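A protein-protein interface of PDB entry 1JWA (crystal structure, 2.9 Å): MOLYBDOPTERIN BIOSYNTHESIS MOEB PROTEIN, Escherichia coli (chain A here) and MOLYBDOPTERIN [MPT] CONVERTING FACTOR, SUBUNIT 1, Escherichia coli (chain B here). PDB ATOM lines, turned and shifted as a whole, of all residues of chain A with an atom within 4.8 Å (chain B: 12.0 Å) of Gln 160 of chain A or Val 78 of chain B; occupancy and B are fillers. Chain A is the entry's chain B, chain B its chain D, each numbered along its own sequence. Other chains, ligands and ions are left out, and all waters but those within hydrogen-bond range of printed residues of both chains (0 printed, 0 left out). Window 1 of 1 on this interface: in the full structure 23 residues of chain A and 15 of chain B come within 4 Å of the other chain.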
ATOM      1  N   SER A 151      16.580  27.034 -16.231  1.00  0.00           N
ATOM      2  CA  SER A 151      16.893  28.090 -17.178  1.00  0.00           C
ATOM      3  C   SER A 151      17.453  27.576 -18.491  1.00  0.00           C
ATOM      4  O   SER A 151      18.278  26.661 -18.503  1.00  0.00           O
ATOM      5  CB  SER A 151      17.890  29.064 -16.558  1.00  0.00           C
ATOM      6  OG  SER A 151      18.161  30.139 -17.432  1.00  0.00           O
ATOM      7  N   GLY A 152      16.995  28.174 -19.594  1.00  0.00           N
ATOM      8  CA  GLY A 152      17.487  27.783 -20.900  1.00  0.00           C
ATOM      9  C   GLY A 152      17.623  28.921 -21.877  1.00  0.00           C
ATOM     10  O   GLY A 152      17.042  29.964 -21.686  1.00  0.00           O
ATOM     11  N   ALA A 153      18.405  28.729 -22.922  1.00  0.00           N
ATOM     12  CA  ALA A 153      18.521  29.783 -23.942  1.00  0.00           C
ATOM     13  C   ALA A 153      18.924  29.206 -25.303  1.00  0.00           C
ATOM     14  O   ALA A 153      19.492  28.123 -25.377  1.00  0.00           O
ATOM     15  CB  ALA A 153      19.511  30.844 -23.515  1.00  0.00           C
ATOM     16  N   ALA A 154      18.631  29.955 -26.361  1.00  0.00           N
ATOM     17  CA  ALA A 154      18.931  29.520 -27.716  1.00  0.00           C
ATOM     18  C   ALA A 154      18.980  30.664 -28.696  1.00  0.00           C
ATOM     19  O   ALA A 154      18.240  31.595 -28.578  1.00  0.00           O
ATOM     20  CB  ALA A 154      17.908  28.515 -28.168  1.00  0.00           C
ATOM     21  N   ILE A 155      19.852  30.580 -29.676  1.00  0.00           N
ATOM     22  CA  ILE A 155      19.939  31.607 -30.689  1.00  0.00           C
ATOM     23  C   ILE A 155      20.737  31.018 -31.830  1.00  0.00           C
ATOM     24  O   ILE A 155      21.561  30.158 -31.601  1.00  0.00           O
ATOM     25  CB  ILE A 155      20.607  32.868 -30.169  1.00  0.00           C
ATOM     26  CG1 ILE A 155      20.260  34.041 -31.078  1.00  0.00           C
ATOM     27  CG2 ILE A 155      22.074  32.714 -30.148  1.00  0.00           C
ATOM     28  CD1 ILE A 155      20.056  35.324 -30.321  1.00  0.00           C
ATOM     29  N   GLU A 158      22.553  27.438 -31.568  1.00  0.00           N
ATOM     30  CA  GLU A 158      23.156  27.046 -30.318  1.00  0.00           C
ATOM     31  C   GLU A 158      22.217  27.168 -29.103  1.00  0.00           C
ATOM     32  O   GLU A 158      21.545  28.162 -28.913  1.00  0.00           O
ATOM     33  CB  GLU A 158      24.385  27.900 -30.091  1.00  0.00           C
ATOM     34  CG  GLU A 158      25.243  27.404 -28.945  1.00  0.00           C
ATOM     35  CD  GLU A 158      26.086  28.498 -28.334  1.00  0.00           C
ATOM     36  OE1 GLU A 158      26.112  29.618 -28.933  1.00  0.00           O
ATOM     37  OE2 GLU A 158      26.689  28.212 -27.251  1.00  0.00           O
ATOM     38  N   GLY A 159      22.222  26.147 -28.264  1.00  0.00           N
ATOM     39  CA  GLY A 159      21.405  26.139 -27.080  1.00  0.00           C
ATOM     40  C   GLY A 159      22.152  25.772 -25.788  1.00  0.00           C
ATOM     41  O   GLY A 159      23.266  25.227 -25.794  1.00  0.00           O
ATOM     42  N   GLN A 160      21.498  26.053 -24.672  1.00  0.00           N
ATOM     43  CA  GLN A 160      22.056  25.784 -23.370  1.00  0.00           C
ATOM     44  C   GLN A 160      20.917  25.522 -22.425  1.00  0.00           C
ATOM     45  O   GLN A 160      19.854  26.085 -22.557  1.00  0.00           O
ATOM     46  CB  GLN A 160      22.810  27.003 -22.843  1.00  0.00           C
ATOM     47  CG  GLN A 160      24.295  26.971 -23.023  1.00  0.00           C
ATOM     48  CD  GLN A 160      24.906  28.389 -23.148  1.00  0.00           C
ATOM     49  OE1 GLN A 160      24.484  29.329 -22.423  1.00  0.00           O
ATOM     50  NE2 GLN A 160      25.880  28.552 -24.075  1.00  0.00           N
ATOM     51  N   ILE A 161      21.173  24.734 -21.407  1.00  0.00           N
ATOM     52  CA  ILE A 161      20.169  24.455 -20.392  1.00  0.00           C
ATOM     53  C   ILE A 161      20.909  24.272 -19.067  1.00  0.00           C
ATOM     54  O   ILE A 161      21.938  23.643 -19.045  1.00  0.00           O
ATOM     55  CB  ILE A 161      19.371  23.180 -20.777  1.00  0.00           C
ATOM     56  CG1 ILE A 161      18.076  23.092 -20.011  1.00  0.00           C
ATOM     57  CG2 ILE A 161      20.169  21.938 -20.482  1.00  0.00           C
ATOM     58  CD1 ILE A 161      18.220  22.774 -18.592  1.00  0.00           C
ATOM     59  N   THR A 162      20.393  24.832 -17.977  1.00  0.00           N
ATOM     60  CA  THR A 162      21.019  24.706 -16.655  1.00  0.00           C
ATOM     61  C   THR A 162      19.964  24.702 -15.606  1.00  0.00           C
ATOM     62  O   THR A 162      18.944  25.386 -15.738  1.00  0.00           O
ATOM     63  CB  THR A 162      21.994  25.893 -16.298  1.00  0.00           C
ATOM     64  OG1 THR A 162      23.144  25.885 -17.169  1.00  0.00           O
ATOM     65  CG2 THR A 162      22.630  25.660 -14.968  1.00  0.00           C
ATOM     66  N   ILE A 200      15.841  22.492 -27.078  1.00  0.00           N
ATOM     67  CA  ILE A 200      16.100  23.096 -25.788  1.00  0.00           C
ATOM     68  C   ILE A 200      14.821  23.191 -24.979  1.00  0.00           C
ATOM     69  O   ILE A 200      14.816  22.945 -23.765  1.00  0.00           O
ATOM     70  CB  ILE A 200      16.686  24.519 -25.964  1.00  0.00           C
ATOM     71  CG1 ILE A 200      18.099  24.451 -26.509  1.00  0.00           C
ATOM     72  CG2 ILE A 200      16.697  25.300 -24.627  1.00  0.00           C
ATOM     73  CD1 ILE A 200      19.110  23.761 -25.558  1.00  0.00           C
ATOM     74  N   ILE A 223      26.199  23.029 -17.240  1.00  0.00           N
ATOM     75  CA  ILE A 223      25.531  23.584 -18.393  1.00  0.00           C
ATOM     76  C   ILE A 223      25.673  22.568 -19.510  1.00  0.00           C
ATOM     77  O   ILE A 223      26.763  22.156 -19.857  1.00  0.00           O
ATOM     78  CB  ILE A 223      26.171  24.927 -18.823  1.00  0.00           C
ATOM     79  CG1 ILE A 223      26.296  25.858 -17.623  1.00  0.00           C
ATOM     80  CG2 ILE A 223      25.419  25.583 -19.864  1.00  0.00           C
ATOM     81  CD1 ILE A 223      27.696  25.687 -16.948  1.00  0.00           C
ATOM     82  N   VAL A 224      24.554  22.153 -20.072  1.00  0.00           N
ATOM     83  CA  VAL A 224      24.579  21.255 -21.208  1.00  0.00           C
ATOM     84  C   VAL A 224      24.419  22.151 -22.400  1.00  0.00           C
ATOM     85  O   VAL A 224      23.458  22.876 -22.478  1.00  0.00           O
ATOM     86  CB  VAL A 224      23.441  20.231 -21.173  1.00  0.00           C
ATOM     87  CG1 VAL A 224      23.574  19.277 -22.353  1.00  0.00           C
ATOM     88  CG2 VAL A 224      23.471  19.462 -19.860  1.00  0.00           C
ATOM     89  N   MET A 225      25.397  22.148 -23.282  1.00  0.00           N
ATOM     90  CA  MET A 225      25.390  22.995 -24.460  1.00  0.00           C
ATOM     91  C   MET A 225      25.123  22.106 -25.643  1.00  0.00           C
ATOM     92  O   MET A 225      25.562  20.954 -25.654  1.00  0.00           O
ATOM     93  CB  MET A 225      26.748  23.677 -24.592  1.00  0.00           C
ATOM     94  CG  MET A 225      26.786  24.800 -25.583  1.00  0.00           C
ATOM     95  SD  MET A 225      27.431  24.180 -27.168  1.00  0.00           S
ATOM     96  CE  MET A 225      29.223  23.939 -26.655  1.00  0.00           C
ATOM     97  N   PHE B   6      37.220  25.035 -30.329  1.00  0.00           N
ATOM     98  CA  PHE B   6      36.244  26.063 -30.704  1.00  0.00           C
ATOM     99  C   PHE B   6      34.875  25.446 -30.947  1.00  0.00           C
ATOM    100  O   PHE B   6      34.746  24.452 -31.635  1.00  0.00           O
ATOM    101  CB  PHE B   6      36.682  26.817 -31.953  1.00  0.00           C
ATOM    102  CG  PHE B   6      37.942  27.594 -31.772  1.00  0.00           C
ATOM    103  CD1 PHE B   6      39.082  27.252 -32.464  1.00  0.00           C
ATOM    104  CD2 PHE B   6      37.992  28.671 -30.902  1.00  0.00           C
ATOM    105  CE1 PHE B   6      40.228  27.965 -32.290  1.00  0.00           C
ATOM    106  CE2 PHE B   6      39.160  29.390 -30.737  1.00  0.00           C
ATOM    107  CZ  PHE B   6      40.266  29.034 -31.423  1.00  0.00           C
ATOM    108  N   PHE B   7      33.857  26.069 -30.371  1.00  0.00           N
ATOM    109  CA  PHE B   7      32.485  25.608 -30.516  1.00  0.00           C
ATOM    110  C   PHE B   7      31.508  26.661 -31.034  1.00  0.00           C
ATOM    111  O   PHE B   7      31.686  27.860 -30.847  1.00  0.00           O
ATOM    112  CB  PHE B   7      31.993  25.052 -29.192  1.00  0.00           C
ATOM    113  CG  PHE B   7      32.525  23.676 -28.893  1.00  0.00           C
ATOM    114  CD1 PHE B   7      33.575  23.500 -27.981  1.00  0.00           C
ATOM    115  CD2 PHE B   7      31.961  22.550 -29.513  1.00  0.00           C
ATOM    116  CE1 PHE B   7      34.042  22.236 -27.693  1.00  0.00           C
ATOM    117  CE2 PHE B   7      32.426  21.259 -29.225  1.00  0.00           C
ATOM    118  CZ  PHE B   7      33.462  21.096 -28.326  1.00  0.00           C
ATOM    119  N   ALA B   8      30.471  26.181 -31.700  1.00  0.00           N
ATOM    120  CA  ALA B   8      29.399  27.020 -32.229  1.00  0.00           C
ATOM    121  C   ALA B   8      29.904  28.117 -33.154  1.00  0.00           C
ATOM    122  O   ALA B   8      30.825  27.947 -33.920  1.00  0.00           O
ATOM    123  CB  ALA B   8      28.552  27.631 -31.069  1.00  0.00           C
ATOM    124  N   GLN B   9      29.264  29.273 -33.062  1.00  0.00           N
ATOM    125  CA  GLN B   9      29.588  30.412 -33.901  1.00  0.00           C
ATOM    126  C   GLN B   9      31.076  30.743 -33.871  1.00  0.00           C
ATOM    127  O   GLN B   9      31.658  31.148 -34.860  1.00  0.00           O
ATOM    128  CB  GLN B   9      28.808  31.627 -33.464  1.00  0.00           C
ATOM    129  CG  GLN B   9      28.419  32.524 -34.627  1.00  0.00           C
ATOM    130  CD  GLN B   9      28.258  33.993 -34.253  1.00  0.00           C
ATOM    131  OE1 GLN B   9      28.764  34.444 -33.235  1.00  0.00           O
ATOM    132  NE2 GLN B   9      27.541  34.739 -35.097  1.00  0.00           N
ATOM    133  N   VAL B  10      31.719  30.578 -32.726  1.00  0.00           N
ATOM    134  CA  VAL B  10      33.131  30.882 -32.661  1.00  0.00           C
ATOM    135  C   VAL B  10      33.881  30.040 -33.689  1.00  0.00           C
ATOM    136  O   VAL B  10      34.588  30.573 -34.517  1.00  0.00           O
ATOM    137  CB  VAL B  10      33.675  30.725 -31.241  1.00  0.00           C
ATOM    138  CG1 VAL B  10      35.179  30.420 -31.256  1.00  0.00           C
ATOM    139  CG2 VAL B  10      33.367  31.991 -30.435  1.00  0.00           C
ATOM    140  N   GLY B  49      33.880  40.377 -24.183  1.00  0.00           N
ATOM    141  CA  GLY B  49      32.502  40.651 -23.817  1.00  0.00           C
ATOM    142  C   GLY B  49      31.527  39.655 -24.420  1.00  0.00           C
ATOM    143  O   GLY B  49      30.508  39.303 -23.808  1.00  0.00           O
ATOM    144  N   LYS B  50      31.846  39.199 -25.627  1.00  0.00           N
ATOM    145  CA  LYS B  50      31.020  38.233 -26.341  1.00  0.00           C
ATOM    146  C   LYS B  50      31.643  36.834 -26.408  1.00  0.00           C
ATOM    147  O   LYS B  50      31.402  36.114 -27.374  1.00  0.00           O
ATOM    148  CB  LYS B  50      30.744  38.713 -27.769  1.00  0.00           C
ATOM    149  CG  LYS B  50      30.812  40.217 -27.985  1.00  0.00           C
ATOM    150  CD  LYS B  50      31.125  40.565 -29.463  1.00  0.00           C
ATOM    151  CE  LYS B  50      29.970  41.337 -30.168  1.00  0.00           C
ATOM    152  NZ  LYS B  50      29.670  42.707 -29.563  1.00  0.00           N
ATOM    153  N   LEU B  51      32.422  36.444 -25.393  1.00  0.00           N
ATOM    154  CA  LEU B  51      33.066  35.133 -25.383  1.00  0.00           C
ATOM    155  C   LEU B  51      33.026  34.458 -24.015  1.00  0.00           C
ATOM    156  O   LEU B  51      32.950  35.118 -22.997  1.00  0.00           O
ATOM    157  CB  LEU B  51      34.510  35.283 -25.845  1.00  0.00           C
ATOM    158  CG  LEU B  51      35.209  33.982 -26.228  1.00  0.00           C
ATOM    159  CD1 LEU B  51      34.503  33.294 -27.402  1.00  0.00           C
ATOM    160  CD2 LEU B  51      36.660  34.245 -26.578  1.00  0.00           C
ATOM    161  N   LEU B  52      33.054  33.137 -24.007  1.00  0.00           N
ATOM    162  CA  LEU B  52      33.035  32.363 -22.784  1.00  0.00           C
ATOM    163  C   LEU B  52      34.163  31.349 -22.846  1.00  0.00           C
ATOM    164  O   LEU B  52      34.333  30.675 -23.867  1.00  0.00           O
ATOM    165  CB  LEU B  52      31.701  31.619 -22.631  1.00  0.00           C
ATOM    166  CG  LEU B  52      30.455  32.406 -22.211  1.00  0.00           C
ATOM    167  CD1 LEU B  52      29.206  31.541 -22.359  1.00  0.00           C
ATOM    168  CD2 LEU B  52      30.602  32.873 -20.803  1.00  0.00           C
ATOM    169  N   ALA B  53      34.903  31.218 -21.745  1.00  0.00           N
ATOM    170  CA  ALA B  53      36.026  30.293 -21.658  1.00  0.00           C
ATOM    171  C   ALA B  53      35.693  29.113 -20.767  1.00  0.00           C
ATOM    172  O   ALA B  53      35.088  29.266 -19.733  1.00  0.00           O
ATOM    173  CB  ALA B  53      37.267  31.029 -21.130  1.00  0.00           C
ATOM    174  N   ALA B  54      36.143  27.935 -21.178  1.00  0.00           N
ATOM    175  CA  ALA B  54      35.946  26.695 -20.440  1.00  0.00           C
ATOM    176  C   ALA B  54      37.267  25.907 -20.332  1.00  0.00           C
ATOM    177  O   ALA B  54      37.731  25.326 -21.312  1.00  0.00           O
ATOM    178  CB  ALA B  54      34.938  25.874 -21.140  1.00  0.00           C
ATOM    179  N   LEU B  59      34.015  25.608 -16.284  1.00  0.00           N
ATOM    180  CA  LEU B  59      34.009  27.010 -16.683  1.00  0.00           C
ATOM    181  C   LEU B  59      34.994  27.789 -15.813  1.00  0.00           C
ATOM    182  O   LEU B  59      35.211  27.430 -14.653  1.00  0.00           O
ATOM    183  CB  LEU B  59      32.624  27.612 -16.518  1.00  0.00           C
ATOM    184  CG  LEU B  59      31.624  27.325 -17.630  1.00  0.00           C
ATOM    185  CD1 LEU B  59      30.354  28.088 -17.338  1.00  0.00           C
ATOM    186  CD2 LEU B  59      32.174  27.712 -18.983  1.00  0.00           C
ATOM    187  N   ALA B  73      38.497  25.557 -24.325  1.00  0.00           N
ATOM    188  CA  ALA B  73      37.458  25.631 -25.334  1.00  0.00           C
ATOM    189  C   ALA B  73      36.851  27.032 -25.308  1.00  0.00           C
ATOM    190  O   ALA B  73      36.637  27.598 -24.250  1.00  0.00           O
ATOM    191  CB  ALA B  73      36.432  24.591 -25.080  1.00  0.00           C
ATOM    192  N   PHE B  74      36.616  27.601 -26.481  1.00  0.00           N
ATOM    193  CA  PHE B  74      36.027  28.936 -26.582  1.00  0.00           C
ATOM    194  C   PHE B  74      34.674  28.933 -27.324  1.00  0.00           C
ATOM    195  O   PHE B  74      34.601  28.771 -28.544  1.00  0.00           O
ATOM    196  CB  PHE B  74      37.005  29.884 -27.288  1.00  0.00           C
ATOM    197  CG  PHE B  74      38.063  30.438 -26.389  1.00  0.00           C
ATOM    198  CD1 PHE B  74      39.401  30.102 -26.568  1.00  0.00           C
ATOM    199  CD2 PHE B  74      37.713  31.317 -25.369  1.00  0.00           C
ATOM    200  CE1 PHE B  74      40.373  30.630 -25.727  1.00  0.00           C
ATOM    201  CE2 PHE B  74      38.662  31.855 -24.531  1.00  0.00           C
ATOM    202  CZ  PHE B  74      39.991  31.523 -24.700  1.00  0.00           C
ATOM    203  N   PHE B  75      33.600  29.107 -26.576  1.00  0.00           N
ATOM    204  CA  PHE B  75      32.270  29.161 -27.181  1.00  0.00           C
ATOM    205  C   PHE B  75      31.575  30.450 -26.769  1.00  0.00           C
ATOM    206  O   PHE B  75      31.935  31.031 -25.765  1.00  0.00           O
ATOM    207  CB  PHE B  75      31.435  27.915 -26.795  1.00  0.00           C
ATOM    208  CG  PHE B  75      31.333  27.673 -25.325  1.00  0.00           C
ATOM    209  CD1 PHE B  75      30.126  27.840 -24.676  1.00  0.00           C
ATOM    210  CD2 PHE B  75      32.437  27.257 -24.591  1.00  0.00           C
ATOM    211  CE1 PHE B  75      30.011  27.614 -23.304  1.00  0.00           C
ATOM    212  CE2 PHE B  75      32.334  27.034 -23.225  1.00  0.00           C
ATOM    213  CZ  PHE B  75      31.113  27.215 -22.579  1.00  0.00           C
ATOM    214  N   PRO B  76      30.592  30.909 -27.533  1.00  0.00           N
ATOM    215  CA  PRO B  76      29.883  32.123 -27.140  1.00  0.00           C
ATOM    216  C   PRO B  76      28.759  31.867 -26.111  1.00  0.00           C
ATOM    217  O   PRO B  76      28.325  30.770 -25.806  1.00  0.00           O
ATOM    218  CB  PRO B  76      29.306  32.654 -28.464  1.00  0.00           C
ATOM    219  CG  PRO B  76      29.328  31.537 -29.407  1.00  0.00           C
ATOM    220  CD  PRO B  76      30.060  30.371 -28.790  1.00  0.00           C
ATOM    221  N   PRO B  77      28.299  32.941 -25.532  1.00  0.00           N
ATOM    222  CA  PRO B  77      27.210  32.847 -24.584  1.00  0.00           C
ATOM    223  C   PRO B  77      25.861  32.955 -25.321  1.00  0.00           C
ATOM    224  O   PRO B  77      25.741  33.604 -26.363  1.00  0.00           O
ATOM    225  CB  PRO B  77      27.468  34.039 -23.649  1.00  0.00           C
ATOM    226  CG  PRO B  77      28.577  34.848 -24.301  1.00  0.00           C
ATOM    227  CD  PRO B  77      28.763  34.324 -25.695  1.00  0.00           C
ATOM    228  N   VAL B  78      24.844  32.315 -24.755  1.00  0.00           N
ATOM    229  CA  VAL B  78      23.519  32.306 -25.359  1.00  0.00           C
ATOM    230  C   VAL B  78      22.422  32.950 -24.483  1.00  0.00           C
ATOM    231  O   VAL B  78      22.290  32.674 -23.327  1.00  0.00           O
ATOM    232  CB  VAL B  78      23.116  30.880 -25.656  1.00  0.00           C
ATOM    233  CG1 VAL B  78      21.988  30.867 -26.645  1.00  0.00           C
ATOM    234  CG2 VAL B  78      24.286  30.118 -26.177  1.00  0.00           C
ATOM    235  N   THR B  79      21.649  33.848 -25.050  1.00  0.00           N
ATOM    236  CA  THR B  79      20.497  34.412 -24.336  1.00  0.00           C
ATOM    237  C   THR B  79      19.484  34.638 -25.440  1.00  0.00           C
ATOM    238  O   THR B  79      19.839  35.045 -26.541  1.00  0.00           O
ATOM    239  CB  THR B  79      20.804  35.717 -23.591  1.00  0.00           C
ATOM    240  OG1 THR B  79      20.651  36.847 -24.451  1.00  0.00           O
ATOM    241  CG2 THR B  79      22.255  35.754 -23.127  1.00  0.00           C
ATOM    242  N   GLY B  80      18.244  34.302 -25.177  1.00  0.00           N
ATOM    243  CA  GLY B  80      17.228  34.428 -26.182  1.00  0.00           C
ATOM    244  C   GLY B  80      16.519  33.126 -26.173  1.00  0.00           C
ATOM    245  O   GLY B  80      17.028  32.183 -25.576  1.00  0.00           O
ATOM    246  N   GLY B  81      15.364  33.075 -26.817  1.00  0.00           N
ATOM    247  CA  GLY B  81      14.568  31.868 -26.879  1.00  0.00           C
ATOM    248  C   GLY B  81      13.375  32.030 -25.986  1.00  0.00           C
ATOM    249  O   GLY B  81      12.414  31.244 -26.129  1.00  0.00           O
ATOM    250  OXT GLY B  81      13.480  32.972 -25.196  1.00  0.00           O
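Gln 160 of chain A touches just these residues of chain B: Pro 76 (3.7 Å) and Val 78 (3.1 Å). No residue of chain B comes within 4 Å of Ser 151 of chain A. Gly 152 of chain A touches none of the printed residues of chain B. Ala 153 of chain A touches three residues of chain B. Of the printed residues of chain B, Ile 155 of chain A touches Val 78 (3.7 Å) and Thr 79 (3.8 Å). Glu 158 of chain A touches three residues of chain B. Gly 159 of chain A touches none of the printed residues of chain B. No residue of chain B comes within 4 Å of Ile 161 of chain A. No residue of chain B comes within 4 Å of Thr 162 of chain A. Ile 223 of chain A touches just one residue of chain B: Leu 59. No residue of chain B comes within 4 Å of Val 224 of chain A. Of chain B, only Phe 7 (3.9 Å) comes within 4 Å of Met 225 of chain A. Of the printed residues of chain A, Gly 81 of chain B touches Ala 154. Of the printed residues of chain A, Gly 80 of chain B touches Ala 153 and Ala 154. The nearest printed residue of chain A that does not touch Phe 7 of chain B is Glu 158 of chain A (6.2 Å).
The backbone carbonyl oxygen (O) of Ala 153 of chain A lies within hydrogen-bond range of the backbone NH (N) of Gln 160 of chain A, at 3.0 Å. The side-chain carboxylate (OE2) of Glu 158 of chain A is in hydrogen-bond range of the side-chain amide nitrogen (NE2) of Gln 160 of chain A. N of Phe 7 of chain B sits at hydrogen-bond distance from O of Phe 74 of chain B, at 3.3 Å.
Hydrophobic or aromatic side chains of chain A within 4 Å of the printed part of chain B: Ala 153, Ile 155, Ile 223 and Met 225. Hydrophobic or aromatic side chains of chain B that line the printed part of chain A: Phe 7, Ala 8, Leu 59, Pro 76 and Val 78. Along chain B the printed residues that touch a printed residue of chain A span positions 7 to 81. Among the printed residues, 15 pairs touch across the chains.
The backbone NH of Ala 154 of chain A is in hydrogen-bond range of the backbone carbonyl oxygen of Gly 80 of chain B. The backbone carbonyl oxygen of Pro 76 of chain B sits close to the side-chain carboxylate of Glu 158 of chain A (3.4 Å).
Among the printed residues, pairs that only touch across the chains: Ala 153 of chain A with Val 78 of chain B, Ala 153 of chain A with Thr 79 of chain B, Ala 153 of chain A with Gly 80 of chain B, Ala 154 of chain A with Val 78 of chain B, Ala 154 of chain A with Gly 81 of chain B, Ile 155 of chain A with Val 78 of chain B, Ile 155 of chain A with Thr 79 of chain B, Glu 158 of chain A with Ala 8 of chain B, Glu 158 of chain A with Val 78 of chain B, Gln 160 of chain A with Pro 76 of chain B, Gln 160 of chain A with Val 78 of chain B, Ile 223 of chain A with Leu 59 of chain B and Met 225 of chain A with Phe 7 of chain B.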
